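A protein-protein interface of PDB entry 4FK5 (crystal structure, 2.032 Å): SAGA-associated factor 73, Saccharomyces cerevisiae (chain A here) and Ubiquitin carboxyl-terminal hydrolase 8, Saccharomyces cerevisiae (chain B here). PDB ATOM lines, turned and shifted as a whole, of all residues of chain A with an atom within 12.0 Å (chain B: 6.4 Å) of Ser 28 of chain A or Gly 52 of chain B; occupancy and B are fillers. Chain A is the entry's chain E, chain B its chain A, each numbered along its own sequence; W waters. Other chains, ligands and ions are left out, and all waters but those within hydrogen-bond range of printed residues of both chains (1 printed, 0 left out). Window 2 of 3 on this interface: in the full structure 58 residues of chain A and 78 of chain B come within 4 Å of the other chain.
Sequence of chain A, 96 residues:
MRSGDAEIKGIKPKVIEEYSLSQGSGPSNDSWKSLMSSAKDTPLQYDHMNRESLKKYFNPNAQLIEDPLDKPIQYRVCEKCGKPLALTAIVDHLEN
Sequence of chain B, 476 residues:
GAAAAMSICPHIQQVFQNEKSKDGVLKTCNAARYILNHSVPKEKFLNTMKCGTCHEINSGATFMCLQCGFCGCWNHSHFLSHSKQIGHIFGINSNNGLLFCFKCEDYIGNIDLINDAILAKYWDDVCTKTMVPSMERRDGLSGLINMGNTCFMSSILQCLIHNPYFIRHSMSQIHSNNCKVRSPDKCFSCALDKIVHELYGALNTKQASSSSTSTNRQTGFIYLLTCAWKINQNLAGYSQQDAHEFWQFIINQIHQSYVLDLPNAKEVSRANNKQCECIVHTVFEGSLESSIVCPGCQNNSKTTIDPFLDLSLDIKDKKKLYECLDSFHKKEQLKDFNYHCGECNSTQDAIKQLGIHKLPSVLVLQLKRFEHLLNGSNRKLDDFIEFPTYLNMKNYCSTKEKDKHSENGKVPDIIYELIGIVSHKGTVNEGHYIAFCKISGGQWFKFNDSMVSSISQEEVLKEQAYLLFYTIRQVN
NZ of Lys 50 of chain B sits close to NE2 of Gln 23 of chain A. The backbone carbonyl oxygen (O) of Gly 52 of chain B is in hydrogen-bond range of the backbone NH (N) of Ser 28 of chain A (2.9 Å). O of Gly 26 of chain A is in hydrogen-bond range of NE2 of His 55 of chain B (3.1 Å).
The backbone NH of Gly 52 of chain B sits at hydrogen-bond distance from the backbone carbonyl oxygen of Cys 71 of chain B (2.7 Å). A ring nitrogen (NE2) of His 55 of chain B is in hydrogen-bond range of the backbone carbonyl oxygen of Thr 53 of chain B (3.5 Å). OG of Ser 28 of chain A sits at hydrogen-bond distance from N of Asp 30 of chain A.
Ser 25 of chain A touches His 55 of chain B. Gly 52 of chain B touches Pro 27 of chain A. CE1 of His 55 of chain B touches N of Ser 28 of chain A (3.9 Å). Trp 32 of chain A touches Phe 70 of chain B.
Of the printed residues of chain B, Gln 23 of chain A touches Lys 50. Of the printed residues of chain B, Ser 25 of chain A touches His 55. Of the printed residues of chain B, Pro 27 of chain A touches Gly 52 (3.6 Å). Of chain B, only Gly 52 and His 55 come within 4 Å of Ser 28 of chain A. Printed residues of chain B within 4 Å of Trp 32 of chain A: Phe 70 (3.8 Å). Lys 33 of chain A touches none of the printed residues of chain B. No residue of chain A comes within 4 Å of Cys 51 of chain B. Gly 52 of chain B touches just these residues of chain A: Pro 27 (3.6 Å) and Ser 28 (2.9 Å). No residue of chain A comes within 4 Å of Thr 53 of chain B. No residue of chain A comes within 4 Å of Cys 54 of chain B. Of the printed residues of chain A, Phe 70 of chain B touches Trp 32. No residue of chain A comes within 4 Å of Gly 72 of chain B. The nearest residue of chain A that does not touch Gly 52 of chain B is Gly 26 of chain A (4.6 Å). The nearest printed residue of chain B that does not touch Trp 32 of chain A is Cys 71 of chain B (4.01 Å).
Hydrophobic or aromatic side chains of chain B that line the printed part of chain A: His 55. Of the 14 printed residues of chain A, 6 touch a printed residue of chain B. Printed residues of chain A that touch a printed residue of chain B: Gln 23, Ser 25, Gly 26, Pro 27, Ser 28 and Trp 32. Among the printed residues, 7 pairs touch across the chains. Among the printed residues, no Asp or Glu carboxylate lies within 4 Å of a Lys or Arg side-chain nitrogen of the other chain.
Water W1 bridges O of Asp 30 of chain A (3.4 Å) and SG of Cys 71 of chain B (3.6 Å).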
ATOM      1  N   SER A  22      -5.211  -8.198  -5.854  1.00  0.00           N
ATOM      2  CA  SER A  22      -3.870  -7.788  -5.328  1.00  0.00           C
ATOM      3  C   SER A  22      -4.004  -6.604  -4.370  1.00  0.00           C
ATOM      4  O   SER A  22      -4.362  -5.503  -4.772  1.00  0.00           O
ATOM      5  CB  SER A  22      -2.904  -7.416  -6.453  1.00  0.00           C
ATOM      6  OG  SER A  22      -2.683  -8.510  -7.317  1.00  0.00           O
ATOM      7  N   GLN A  23      -3.735  -6.852  -3.101  1.00  0.00           N
ATOM      8  CA  GLN A  23      -3.917  -5.849  -2.063  1.00  0.00           C
ATOM      9  C   GLN A  23      -2.666  -5.844  -1.160  1.00  0.00           C
ATOM     10  O   GLN A  23      -2.365  -6.848  -0.500  1.00  0.00           O
ATOM     11  CB  GLN A  23      -5.199  -6.160  -1.236  1.00  0.00           C
ATOM     12  CG  GLN A  23      -6.528  -6.088  -2.032  1.00  0.00           C
ATOM     13  CD  GLN A  23      -7.737  -6.713  -1.287  1.00  0.00           C
ATOM     14  OE1 GLN A  23      -8.729  -7.128  -1.917  1.00  0.00           O
ATOM     15  NE2 GLN A  23      -7.657  -6.768   0.055  1.00  0.00           N
ATOM     16  N   GLY A  24      -1.916  -4.741  -1.177  1.00  0.00           N
ATOM     17  CA  GLY A  24      -0.765  -4.582  -0.276  1.00  0.00           C
ATOM     18  C   GLY A  24      -1.147  -4.884   1.173  1.00  0.00           C
ATOM     19  O   GLY A  24      -1.932  -4.147   1.779  1.00  0.00           O
ATOM     20  N   SER A  25      -0.590  -5.965   1.733  1.00  0.00           N
ATOM     21  CA  SER A  25      -1.125  -6.544   2.983  1.00  0.00           C
ATOM     22  C   SER A  25      -0.570  -5.875   4.270  1.00  0.00           C
ATOM     23  O   SER A  25      -0.643  -6.456   5.361  1.00  0.00           O
ATOM     24  CB  SER A  25      -0.900  -8.069   3.026  1.00  0.00           C
ATOM     25  OG  SER A  25       0.242  -8.408   3.789  1.00  0.00           O
ATOM     26  N   GLY A  26      -0.061  -4.646   4.141  1.00  0.00           N
ATOM     27  CA  GLY A  26       0.046  -3.744   5.290  1.00  0.00           C
ATOM     28  C   GLY A  26      -1.337  -3.395   5.867  1.00  0.00           C
ATOM     29  O   GLY A  26      -2.374  -3.756   5.290  1.00  0.00           O
ATOM     30  N   PRO A  27      -1.361  -2.686   7.004  1.00  0.00           N
ATOM     31  CA  PRO A  27      -2.643  -2.387   7.668  1.00  0.00           C
ATOM     32  C   PRO A  27      -3.556  -1.541   6.766  1.00  0.00           C
ATOM     33  O   PRO A  27      -3.062  -0.742   5.979  1.00  0.00           O
ATOM     34  CB  PRO A  27      -2.219  -1.592   8.916  1.00  0.00           C
ATOM     35  CG  PRO A  27      -0.726  -1.832   9.062  1.00  0.00           C
ATOM     36  CD  PRO A  27      -0.222  -2.034   7.672  1.00  0.00           C
ATOM     37  N   SER A  28      -4.870  -1.745   6.852  1.00  0.00           N
ATOM     38  CA  SER A  28      -5.808  -1.004   5.989  1.00  0.00           C
ATOM     39  C   SER A  28      -5.887   0.477   6.395  1.00  0.00           C
ATOM     40  O   SER A  28      -5.797   0.793   7.567  1.00  0.00           O
ATOM     41  CB  SER A  28      -7.221  -1.618   6.057  1.00  0.00           C
ATOM     42  OG  SER A  28      -8.171  -0.707   5.536  1.00  0.00           O
ATOM     43  N   ASN A  29      -6.149   1.361   5.429  1.00  0.00           N
ATOM     44  CA  ASN A  29      -6.476   2.779   5.745  1.00  0.00           C
ATOM     45  C   ASN A  29      -7.995   3.111   5.777  1.00  0.00           C
ATOM     46  O   ASN A  29      -8.376   4.265   5.882  1.00  0.00           O
ATOM     47  CB  ASN A  29      -5.752   3.705   4.782  1.00  0.00           C
ATOM     48  CG  ASN A  29      -4.282   3.788   5.083  1.00  0.00           C
ATOM     49  OD1 ASN A  29      -3.875   3.825   6.256  1.00  0.00           O
ATOM     50  ND2 ASN A  29      -3.460   3.773   4.038  1.00  0.00           N
ATOM     51  N   ASP A  30      -8.841   2.085   5.728  1.00  0.00           N
ATOM     52  CA  ASP A  30     -10.290   2.310   5.662  1.00  0.00           C
ATOM     53  C   ASP A  30     -10.828   2.869   6.951  1.00  0.00           C
ATOM     54  O   ASP A  30     -10.250   2.676   8.022  1.00  0.00           O
ATOM     55  CB  ASP A  30     -11.026   1.019   5.320  1.00  0.00           C
ATOM     56  CG  ASP A  30     -10.694   0.517   3.929  1.00  0.00           C
ATOM     57  OD1 ASP A  30     -10.527   1.369   3.008  1.00  0.00           O
ATOM     58  OD2 ASP A  30     -10.573  -0.718   3.762  1.00  0.00           O
ATOM     59  N   SER A  31     -11.975   3.533   6.847  1.00  0.00           N
ATOM     60  CA  SER A  31     -12.700   3.942   7.994  1.00  0.00           C
ATOM     61  C   SER A  31     -14.157   3.516   7.890  1.00  0.00           C
ATOM     62  O   SER A  31     -14.808   3.874   6.968  1.00  0.00           O
ATOM     63  CB  SER A  31     -12.648   5.424   8.115  1.00  0.00           C
ATOM     64  OG  SER A  31     -13.547   5.830   9.083  1.00  0.00           O
ATOM     65  N   TRP A  32     -14.687   2.842   8.897  1.00  0.00           N
ATOM     66  CA  TRP A  32     -16.168   2.562   8.905  1.00  0.00           C
ATOM     67  C   TRP A  32     -16.973   3.825   8.986  1.00  0.00           C
ATOM     68  O   TRP A  32     -18.123   3.886   8.522  1.00  0.00           O
ATOM     69  CB  TRP A  32     -16.518   1.592  10.011  1.00  0.00           C
ATOM     70  CG  TRP A  32     -16.426   2.184  11.431  1.00  0.00           C
ATOM     71  CD1 TRP A  32     -15.401   2.002  12.372  1.00  0.00           C
ATOM     72  CD2 TRP A  32     -17.443   2.956  12.099  1.00  0.00           C
ATOM     73  NE1 TRP A  32     -15.707   2.650  13.560  1.00  0.00           N
ATOM     74  CE2 TRP A  32     -16.948   3.221  13.464  1.00  0.00           C
ATOM     75  CE3 TRP A  32     -18.699   3.415  11.740  1.00  0.00           C
ATOM     76  CZ2 TRP A  32     -17.661   3.966  14.364  1.00  0.00           C
ATOM     77  CZ3 TRP A  32     -19.415   4.190  12.659  1.00  0.00           C
ATOM     78  CH2 TRP A  32     -18.930   4.421  13.960  1.00  0.00           C
ATOM     79  N   LYS A  33     -16.388   4.889   9.526  1.00  0.00           N
ATOM     80  CA  LYS A  33     -17.119   6.172   9.652  1.00  0.00           C
ATOM     81  C   LYS A  33     -17.386   6.807   8.283  1.00  0.00           C
ATOM     82  O   LYS A  33     -18.324   7.605   8.131  1.00  0.00           O
ATOM     83  CB  LYS A  33     -16.373   7.149  10.559  1.00  0.00           C
ATOM     84  CG  LYS A  33     -16.208   6.649  11.978  1.00  0.00           C
ATOM     85  CD  LYS A  33     -15.680   7.719  12.908  1.00  0.00           C
ATOM     86  CE  LYS A  33     -15.102   7.115  14.184  1.00  0.00           C
ATOM     87  NZ  LYS A  33     -15.430   7.909  15.402  1.00  0.00           N
ATOM     88  N   SER A  34     -16.668   6.346   7.268  1.00  0.00           N
ATOM     89  CA  SER A  34     -16.846   6.870   5.895  1.00  0.00           C
ATOM     90  C   SER A  34     -18.114   6.287   5.211  1.00  0.00           C
ATOM     91  O   SER A  34     -18.441   6.660   4.082  1.00  0.00           O
ATOM     92  CB  SER A  34     -15.631   6.517   5.030  1.00  0.00           C
ATOM     93  OG  SER A  34     -15.669   5.104   4.645  1.00  0.00           O
ATOM     94  N   LEU A  35     -18.751   5.318   5.855  1.00  0.00           N
ATOM     95  CA  LEU A  35     -19.918   4.635   5.273  1.00  0.00           C
ATOM     96  C   LEU A  35     -21.203   5.454   5.418  1.00  0.00           C
ATOM     97  O   LEU A  35     -22.231   5.072   4.911  1.00  0.00           O
ATOM     98  CB  LEU A  35     -20.106   3.244   5.913  1.00  0.00           C
ATOM     99  CG  LEU A  35     -18.981   2.271   5.613  1.00  0.00           C
ATOM    100  CD1 LEU A  35     -19.058   1.038   6.533  1.00  0.00           C
ATOM    101  CD2 LEU A  35     -19.031   1.866   4.140  1.00  0.00           C
ATOM    102  N   LYS B  50     -14.565  -6.922   7.836  1.00  0.00           N
ATOM    103  CA  LYS B  50     -13.245  -7.210   7.246  1.00  0.00           C
ATOM    104  C   LYS B  50     -12.192  -6.638   8.185  1.00  0.00           C
ATOM    105  O   LYS B  50     -12.220  -5.460   8.506  1.00  0.00           O
ATOM    106  CB  LYS B  50     -13.111  -6.554   5.885  1.00  0.00           C
ATOM    107  CG  LYS B  50     -11.727  -6.789   5.237  1.00  0.00           C
ATOM    108  CD  LYS B  50     -11.511  -5.874   4.057  1.00  0.00           C
ATOM    109  CE  LYS B  50     -10.975  -6.627   2.844  1.00  0.00           C
ATOM    110  NZ  LYS B  50      -9.944  -5.814   2.110  1.00  0.00           N
ATOM    111  N   CYS B  51     -11.305  -7.481   8.677  1.00  0.00           N
ATOM    112  CA  CYS B  51     -10.318  -7.031   9.663  1.00  0.00           C
ATOM    113  C   CYS B  51      -9.294  -6.098   8.989  1.00  0.00           C
ATOM    114  O   CYS B  51      -8.705  -6.444   7.978  1.00  0.00           O
ATOM    115  CB  CYS B  51      -9.604  -8.228  10.280  1.00  0.00           C
ATOM    116  SG  CYS B  51      -8.383  -7.717  11.549  1.00  0.00           S
ATOM    117  N   GLY B  52      -9.074  -4.940   9.556  1.00  0.00           N
ATOM    118  CA  GLY B  52      -8.043  -4.030   8.988  1.00  0.00           C
ATOM    119  C   GLY B  52      -6.564  -4.541   9.068  1.00  0.00           C
ATOM    120  O   GLY B  52      -5.728  -4.063   8.360  1.00  0.00           O
ATOM    121  N   THR B  53      -6.293  -5.518   9.931  1.00  0.00           N
ATOM    122  CA  THR B  53      -4.946  -6.062  10.096  1.00  0.00           C
ATOM    123  C   THR B  53      -4.752  -7.290   9.188  1.00  0.00           C
ATOM    124  O   THR B  53      -3.910  -7.257   8.335  1.00  0.00           O
ATOM    125  CB  THR B  53      -4.682  -6.413  11.549  1.00  0.00           C
ATOM    126  OG1 THR B  53      -4.937  -5.268  12.357  1.00  0.00           O
ATOM    127  CG2 THR B  53      -3.202  -6.858  11.768  1.00  0.00           C
ATOM    128  N   CYS B  54      -5.586  -8.337   9.317  1.00  0.00           N
ATOM    129  CA  CYS B  54      -5.426  -9.553   8.472  1.00  0.00           C
ATOM    130  C   CYS B  54      -6.265  -9.533   7.198  1.00  0.00           C
ATOM    131  O   CYS B  54      -6.128 -10.424   6.359  1.00  0.00           O
ATOM    132  CB  CYS B  54      -5.724 -10.855   9.275  1.00  0.00           C
ATOM    133  SG  CYS B  54      -7.421 -10.962  10.051  1.00  0.00           S
ATOM    134  N   HIS B  55      -7.214  -8.583   7.085  1.00  0.00           N
ATOM    135  CA  HIS B  55      -8.097  -8.500   5.880  1.00  0.00           C
ATOM    136  C   HIS B  55      -9.071  -9.704   5.673  1.00  0.00           C
ATOM    137  O   HIS B  55      -9.646  -9.867   4.603  1.00  0.00           O
ATOM    138  CB  HIS B  55      -7.240  -8.282   4.611  1.00  0.00           C
ATOM    139  CG  HIS B  55      -6.161  -7.271   4.795  1.00  0.00           C
ATOM    140  ND1 HIS B  55      -6.421  -5.964   5.058  1.00  0.00           N
ATOM    141  CD2 HIS B  55      -4.759  -7.402   4.791  1.00  0.00           C
ATOM    142  CE1 HIS B  55      -5.273  -5.296   5.189  1.00  0.00           C
ATOM    143  NE2 HIS B  55      -4.248  -6.180   5.047  1.00  0.00           N
ATOM    144  N   GLU B  56      -9.192 -10.572   6.659  1.00  0.00           N
ATOM    145  CA  GLU B  56     -10.154 -11.667   6.581  1.00  0.00           C
ATOM    146  C   GLU B  56     -11.570 -11.147   6.827  1.00  0.00           C
ATOM    147  O   GLU B  56     -11.786 -10.228   7.628  1.00  0.00           O
ATOM    148  CB  GLU B  56      -9.848 -12.734   7.609  1.00  0.00           C
ATOM    149  CG  GLU B  56      -8.792 -13.741   7.186  1.00  0.00           C
ATOM    150  CD  GLU B  56      -8.568 -14.847   8.241  1.00  0.00           C
ATOM    151  OE1 GLU B  56      -7.380 -15.192   8.504  1.00  0.00           O
ATOM    152  OE2 GLU B  56      -9.560 -15.415   8.774  1.00  0.00           O
ATOM    153  N   THR B  62     -16.158  -9.015  14.169  1.00  0.00           N
ATOM    154  CA  THR B  62     -15.363  -7.867  13.803  1.00  0.00           C
ATOM    155  C   THR B  62     -15.920  -6.661  14.562  1.00  0.00           C
ATOM    156  O   THR B  62     -17.177  -6.446  14.674  1.00  0.00           O
ATOM    157  CB  THR B  62     -15.344  -7.676  12.262  1.00  0.00           C
ATOM    158  OG1 THR B  62     -14.902  -8.904  11.619  1.00  0.00           O
ATOM    159  CG2 THR B  62     -14.442  -6.574  11.830  1.00  0.00           C
ATOM    160  N   PHE B  70     -11.051   2.214  12.402  1.00  0.00           N
ATOM    161  CA  PHE B  70     -10.514   0.880  12.307  1.00  0.00           C
ATOM    162  C   PHE B  70     -11.599  -0.172  12.611  1.00  0.00           C
ATOM    163  O   PHE B  70     -12.361  -0.022  13.556  1.00  0.00           O
ATOM    164  CB  PHE B  70      -9.357   0.742  13.335  1.00  0.00           C
ATOM    165  CG  PHE B  70      -8.733  -0.623  13.397  1.00  0.00           C
ATOM    166  CD1 PHE B  70      -7.830  -1.042  12.428  1.00  0.00           C
ATOM    167  CD2 PHE B  70      -8.969  -1.460  14.495  1.00  0.00           C
ATOM    168  CE1 PHE B  70      -7.221  -2.271  12.526  1.00  0.00           C
ATOM    169  CE2 PHE B  70      -8.411  -2.698  14.562  1.00  0.00           C
ATOM    170  CZ  PHE B  70      -7.543  -3.124  13.571  1.00  0.00           C
ATOM    171  N   CYS B  71     -11.556  -1.275  11.876  1.00  0.00           N
ATOM    172  CA  CYS B  71     -12.263  -2.531  12.252  1.00  0.00           C
ATOM    173  C   CYS B  71     -11.239  -3.646  12.486  1.00  0.00           C
ATOM    174  O   CYS B  71     -10.300  -3.797  11.703  1.00  0.00           O
ATOM    175  CB  CYS B  71     -13.233  -2.984  11.131  1.00  0.00           C
ATOM    176  SG  CYS B  71     -14.536  -1.808  10.780  1.00  0.00           S
ATOM    177  N   GLY B  72     -11.476  -4.463  13.530  1.00  0.00           N
ATOM    178  CA  GLY B  72     -10.529  -5.521  13.908  1.00  0.00           C
ATOM    179  C   GLY B  72     -11.186  -6.789  14.378  1.00  0.00           C
ATOM    180  O   GLY B  72     -12.198  -6.745  15.073  1.00  0.00           O
ATOM    181  N   CYS B  73     -10.610  -7.938  14.001  1.00  0.00           N
ATOM    182  CA  CYS B  73     -11.218  -9.264  14.313  1.00  0.00           C
ATOM    183  C   CYS B  73     -10.981  -9.741  15.749  1.00  0.00           C
ATOM    184  O   CYS B  73     -10.063  -9.286  16.459  1.00  0.00           O
ATOM    185  CB  CYS B  73     -10.740 -10.339  13.354  1.00  0.00           C
ATOM    186  SG  CYS B  73      -8.952 -10.839  13.557  1.00  0.00           S
HETATM  187  O   HOH W   1     -12.403   0.136   8.649  1.00  0.00           O
